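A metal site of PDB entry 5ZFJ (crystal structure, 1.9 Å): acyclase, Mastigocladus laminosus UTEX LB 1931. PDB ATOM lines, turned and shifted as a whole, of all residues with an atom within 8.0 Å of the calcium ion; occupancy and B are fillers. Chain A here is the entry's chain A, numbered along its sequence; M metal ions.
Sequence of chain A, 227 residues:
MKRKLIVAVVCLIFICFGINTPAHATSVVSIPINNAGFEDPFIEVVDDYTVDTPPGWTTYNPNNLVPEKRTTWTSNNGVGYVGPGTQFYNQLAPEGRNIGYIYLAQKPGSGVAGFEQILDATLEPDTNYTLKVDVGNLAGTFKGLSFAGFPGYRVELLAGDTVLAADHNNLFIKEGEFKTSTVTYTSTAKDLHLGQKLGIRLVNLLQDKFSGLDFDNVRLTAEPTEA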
ATOM      1  N   ASN A  35      -7.868  27.845  -9.439  1.00  0.00           N
ATOM      2  CA  ASN A  35      -9.253  28.031  -9.007  1.00  0.00           C
ATOM      3  C   ASN A  35      -9.545  27.116  -7.813  1.00  0.00           C
ATOM      4  O   ASN A  35     -10.578  26.462  -7.733  1.00  0.00           O
ATOM      5  CB  ASN A  35     -10.247  27.786 -10.152  1.00  0.00           C
ATOM      6  CG  ASN A  35     -11.576  28.487  -9.920  1.00  0.00           C
ATOM      7  OD1 ASN A  35     -11.676  29.391  -9.094  1.00  0.00           O
ATOM      8  ND2 ASN A  35     -12.614  28.032 -10.601  1.00  0.00           N
ATOM      9  N   ALA A  36      -8.618  27.140  -6.851  1.00  0.00           N
ATOM     10  CA  ALA A  36      -8.571  26.159  -5.773  1.00  0.00           C
ATOM     11  C   ALA A  36      -9.713  26.363  -4.784  1.00  0.00           C
ATOM     12  O   ALA A  36     -10.031  25.437  -4.044  1.00  0.00           O
ATOM     13  CB  ALA A  36      -7.210  26.189  -5.113  1.00  0.00           C
ATOM     14  N   GLY A  37     -10.303  27.578  -4.773  1.00  0.00           N
ATOM     15  CA  GLY A  37     -11.446  27.879  -3.948  1.00  0.00           C
ATOM     16  C   GLY A  37     -12.725  28.161  -4.724  1.00  0.00           C
ATOM     17  O   GLY A  37     -13.684  28.690  -4.163  1.00  0.00           O
ATOM     18  N   PHE A  38     -12.735  27.762  -6.014  1.00  0.00           N
ATOM     19  CA  PHE A  38     -13.894  27.912  -6.863  1.00  0.00           C
ATOM     20  C   PHE A  38     -14.388  29.369  -6.900  1.00  0.00           C
ATOM     21  O   PHE A  38     -15.567  29.613  -7.094  1.00  0.00           O
ATOM     22  CB  PHE A  38     -15.002  26.956  -6.394  1.00  0.00           C
ATOM     23  CG  PHE A  38     -14.585  25.501  -6.430  1.00  0.00           C
ATOM     24  CD1 PHE A  38     -14.487  24.832  -7.645  1.00  0.00           C
ATOM     25  CD2 PHE A  38     -14.249  24.812  -5.285  1.00  0.00           C
ATOM     26  CE1 PHE A  38     -14.101  23.499  -7.708  1.00  0.00           C
ATOM     27  CE2 PHE A  38     -13.862  23.478  -5.348  1.00  0.00           C
ATOM     28  CZ  PHE A  38     -13.805  22.811  -6.552  1.00  0.00           C
ATOM     29  N   GLU A  39     -13.483  30.339  -6.778  1.00  0.00           N
ATOM     30  CA  GLU A  39     -13.874  31.744  -6.694  1.00  0.00           C
ATOM     31  C   GLU A  39     -14.144  32.325  -8.091  1.00  0.00           C
ATOM     32  O   GLU A  39     -14.848  33.337  -8.196  1.00  0.00           O
ATOM     33  CB  GLU A  39     -12.848  32.518  -5.875  1.00  0.00           C
ATOM     34  CG  GLU A  39     -12.831  32.113  -4.415  1.00  0.00           C
ATOM     35  CD  GLU A  39     -14.149  32.336  -3.711  1.00  0.00           C
ATOM     36  OE1 GLU A  39     -14.670  33.480  -3.756  1.00  0.00           O
ATOM     37  OE2 GLU A  39     -14.672  31.370  -3.104  1.00  0.00           O
ATOM     38  N   ASP A  40     -13.781  31.579  -9.146  1.00  0.00           N
ATOM     39  CA  ASP A  40     -14.239  31.862 -10.502  1.00  0.00           C
ATOM     40  C   ASP A  40     -15.262  30.828 -10.951  1.00  0.00           C
ATOM     41  O   ASP A  40     -14.999  29.642 -10.818  1.00  0.00           O
ATOM     42  CB  ASP A  40     -13.092  31.840 -11.513  1.00  0.00           C
ATOM     43  CG  ASP A  40     -12.283  33.132 -11.542  1.00  0.00           C
ATOM     44  OD1 ASP A  40     -12.661  34.073 -10.809  1.00  0.00           O
ATOM     45  OD2 ASP A  40     -11.318  33.217 -12.318  1.00  0.00           O
ATOM     46  N   GLY A  80     -21.215  27.717  -6.431  1.00  0.00           N
ATOM     47  CA  GLY A  80     -22.405  28.231  -5.718  1.00  0.00           C
ATOM     48  C   GLY A  80     -21.937  29.227  -4.673  1.00  0.00           C
ATOM     49  O   GLY A  80     -20.923  28.985  -4.024  1.00  0.00           O
ATOM     50  N   VAL A  82     -22.057  30.837  -1.284  1.00  0.00           N
ATOM     51  CA  VAL A  82     -22.506  30.586   0.095  1.00  0.00           C
ATOM     52  C   VAL A  82     -22.190  31.857   0.898  1.00  0.00           C
ATOM     53  O   VAL A  82     -21.085  32.019   1.418  1.00  0.00           O
ATOM     54  CB  VAL A  82     -21.836  29.365   0.753  1.00  0.00           C
ATOM     55  CG1 VAL A  82     -22.362  29.166   2.165  1.00  0.00           C
ATOM     56  CG2 VAL A  82     -22.024  28.089  -0.058  1.00  0.00           C
ATOM     57  N   ALA A  93     -19.095  30.125   3.199  1.00  0.00           N
ATOM     58  CA  ALA A  93     -18.118  29.299   2.494  1.00  0.00           C
ATOM     59  C   ALA A  93     -16.872  29.199   3.355  1.00  0.00           C
ATOM     60  O   ALA A  93     -16.469  30.181   3.986  1.00  0.00           O
ATOM     61  CB  ALA A  93     -17.787  29.887   1.148  1.00  0.00           C
ATOM     62  N   PRO A  94     -16.219  28.011   3.410  1.00  0.00           N
ATOM     63  CA  PRO A  94     -14.923  27.860   4.083  1.00  0.00           C
ATOM     64  C   PRO A  94     -13.893  28.914   3.635  1.00  0.00           C
ATOM     65  O   PRO A  94     -13.070  29.363   4.443  1.00  0.00           O
ATOM     66  CB  PRO A  94     -14.490  26.440   3.688  1.00  0.00           C
ATOM     67  CG  PRO A  94     -15.801  25.710   3.501  1.00  0.00           C
ATOM     68  CD  PRO A  94     -16.752  26.742   2.901  1.00  0.00           C
ATOM     69  N   GLU A  95     -13.975  29.336   2.369  1.00  0.00           N
ATOM     70  CA  GLU A  95     -13.045  30.288   1.837  1.00  0.00           C
ATOM     71  C   GLU A  95     -13.736  31.196   0.805  1.00  0.00           C
ATOM     72  O   GLU A  95     -14.430  30.731  -0.070  1.00  0.00           O
ATOM     73  CB  GLU A  95     -11.857  29.552   1.247  1.00  0.00           C
ATOM     74  CG  GLU A  95     -10.854  30.420   0.507  1.00  0.00           C
ATOM     75  CD  GLU A  95     -11.170  30.725  -0.951  1.00  0.00           C
ATOM     76  OE1 GLU A  95     -10.437  31.584  -1.492  1.00  0.00           O
ATOM     77  OE2 GLU A  95     -12.081  30.110  -1.562  1.00  0.00           O
ATOM     78  N   GLY A  96     -13.535  32.509   0.932  1.00  0.00           N
ATOM     79  CA  GLY A  96     -14.136  33.467  -0.022  1.00  0.00           C
ATOM     80  C   GLY A  96     -15.658  33.357  -0.079  1.00  0.00           C
ATOM     81  O   GLY A  96     -16.349  33.154   0.929  1.00  0.00           O
ATOM     82  N   ARG A  97     -16.192  33.479  -1.300  1.00  0.00           N
ATOM     83  CA  ARG A  97     -17.619  33.565  -1.540  1.00  0.00           C
ATOM     84  C   ARG A  97     -18.212  32.204  -1.924  1.00  0.00           C
ATOM     85  O   ARG A  97     -19.359  31.890  -1.545  1.00  0.00           O
ATOM     86  CB  ARG A  97     -17.863  34.541  -2.701  1.00  0.00           C
ATOM     87  CG  ARG A  97     -17.563  35.999  -2.390  1.00  0.00           C
ATOM     88  CD  ARG A  97     -17.613  36.844  -3.648  1.00  0.00           C
ATOM     89  NE  ARG A  97     -18.972  37.040  -4.151  1.00  0.00           N
ATOM     90  CZ  ARG A  97     -19.762  38.039  -3.800  1.00  0.00           C
ATOM     91  NH1 ARG A  97     -19.360  38.970  -2.937  1.00  0.00           N
ATOM     92  NH2 ARG A  97     -20.971  38.105  -4.347  1.00  0.00           N
ATOM     93  N   ASN A  98     -17.465  31.432  -2.712  1.00  0.00           N
ATOM     94  CA  ASN A  98     -18.074  30.310  -3.430  1.00  0.00           C
ATOM     95  C   ASN A  98     -17.602  28.965  -2.888  1.00  0.00           C
ATOM     96  O   ASN A  98     -16.482  28.842  -2.361  1.00  0.00           O
ATOM     97  CB  ASN A  98     -17.686  30.283  -4.904  1.00  0.00           C
ATOM     98  CG  ASN A  98     -18.242  31.455  -5.704  1.00  0.00           C
ATOM     99  OD1 ASN A  98     -19.145  32.165  -5.247  1.00  0.00           O
ATOM    100  ND2 ASN A  98     -17.667  31.671  -6.876  1.00  0.00           N
ATOM    101  N   ILE A  99     -18.414  27.950  -3.230  1.00  0.00           N
ATOM    102  CA  ILE A  99     -18.015  26.558  -3.152  1.00  0.00           C
ATOM    103  C   ILE A  99     -18.164  25.919  -4.532  1.00  0.00           C
ATOM    104  O   ILE A  99     -18.709  26.549  -5.427  1.00  0.00           O
ATOM    105  CB  ILE A  99     -18.844  25.851  -2.063  1.00  0.00           C
ATOM    106  CG1 ILE A  99     -20.348  25.831  -2.351  1.00  0.00           C
ATOM    107  CG2 ILE A  99     -18.538  26.521  -0.732  1.00  0.00           C
ATOM    108  CD1 ILE A  99     -20.772  24.898  -3.463  1.00  0.00           C
ATOM    109  N   GLY A 100     -17.538  24.758  -4.722  1.00  0.00           N
ATOM    110  CA  GLY A 100     -17.797  23.900  -5.921  1.00  0.00           C
ATOM    111  C   GLY A 100     -18.735  22.775  -5.523  1.00  0.00           C
ATOM    112  O   GLY A 100     -18.483  22.076  -4.532  1.00  0.00           O
ATOM    113  N   PHE A 215     -17.558  21.299  -2.131  1.00  0.00           N
ATOM    114  CA  PHE A 215     -16.163  21.321  -1.785  1.00  0.00           C
ATOM    115  C   PHE A 215     -15.657  22.756  -1.747  1.00  0.00           C
ATOM    116  O   PHE A 215     -16.186  23.609  -2.459  1.00  0.00           O
ATOM    117  CB  PHE A 215     -15.328  20.534  -2.789  1.00  0.00           C
ATOM    118  CG  PHE A 215     -15.643  19.068  -2.846  1.00  0.00           C
ATOM    119  CD1 PHE A 215     -15.113  18.199  -1.905  1.00  0.00           C
ATOM    120  CD2 PHE A 215     -16.514  18.556  -3.801  1.00  0.00           C
ATOM    121  CE1 PHE A 215     -15.388  16.843  -1.946  1.00  0.00           C
ATOM    122  CE2 PHE A 215     -16.802  17.190  -3.830  1.00  0.00           C
ATOM    123  CZ  PHE A 215     -16.238  16.342  -2.903  1.00  0.00           C
ATOM    124  N   ASP A 216     -14.612  23.017  -0.943  1.00  0.00           N
ATOM    125  CA  ASP A 216     -13.986  24.338  -0.980  1.00  0.00           C
ATOM    126  C   ASP A 216     -12.554  24.252  -0.445  1.00  0.00           C
ATOM    127  O   ASP A 216     -12.159  23.346   0.273  1.00  0.00           O
ATOM    128  CB  ASP A 216     -14.789  25.420  -0.250  1.00  0.00           C
ATOM    129  CG  ASP A 216     -14.455  26.853  -0.671  1.00  0.00           C
ATOM    130  OD1 ASP A 216     -13.711  27.061  -1.672  1.00  0.00           O
ATOM    131  OD2 ASP A 216     -14.917  27.809  -0.006  1.00  0.00           O
ATOM    132  N   ASN A 217     -11.780  25.281  -0.805  1.00  0.00           N
ATOM    133  CA  ASN A 217     -10.485  25.576  -0.202  1.00  0.00           C
ATOM    134  C   ASN A 217      -9.534  24.385  -0.345  1.00  0.00           C
ATOM    135  O   ASN A 217      -9.000  23.902   0.644  1.00  0.00           O
ATOM    136  CB  ASN A 217     -10.616  25.915   1.291  1.00  0.00           C
ATOM    137  CG  ASN A 217      -9.378  26.600   1.822  1.00  0.00           C
ATOM    138  OD1 ASN A 217      -8.530  27.049   1.056  1.00  0.00           O
ATOM    139  ND2 ASN A 217      -9.239  26.596   3.132  1.00  0.00           N
ATOM    140  N   VAL A 218      -9.328  23.930  -1.587  1.00  0.00           N
ATOM    141  CA  VAL A 218      -8.431  22.853  -1.851  1.00  0.00           C
ATOM    142  C   VAL A 218      -7.010  23.361  -1.643  1.00  0.00           C
ATOM    143  O   VAL A 218      -6.591  24.387  -2.188  1.00  0.00           O
ATOM    144  CB  VAL A 218      -8.610  22.321  -3.285  1.00  0.00           C
ATOM    145  CG1 VAL A 218      -7.750  21.112  -3.547  1.00  0.00           C
ATOM    146  CG2 VAL A 218     -10.071  22.054  -3.605  1.00  0.00           C
HETATM  147 CA    CA M   1     -14.278  29.348  -1.934  1.00  0.00          CA
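Within 4 Å of the calcium ion: Gly 37, Glu 39, Glu 95, Asn 98 and Asp 216.
The calcium ion is bound by the backbone carbonyl oxygen (O) of Asn 98, the backbone carbonyl oxygen (O) of Glu 95, the side-chain carboxylate (OE2) of Glu 95, the side-chain carboxylate (OE2) of Glu 39, the side-chain carboxylate (OD1) of Asp 216, the backbone carbonyl oxygen (O) of Gly 37 and the side-chain carboxylate (OD2) of Asp 216.
The backbone NH of Glu 39 is in hydrogen-bond range of the side-chain amide oxygen of Asn 35 (3.1 Å). The side-chain amide nitrogen (ND2) of Asn 98 sits at hydrogen-bond distance from the backbone carbonyl oxygen (O) of Phe 38 (2.9 Å). The side-chain carboxylate (OE1) of Glu 39 lies within hydrogen-bond range of the backbone NH (N) of Arg 97 (2.9 Å).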
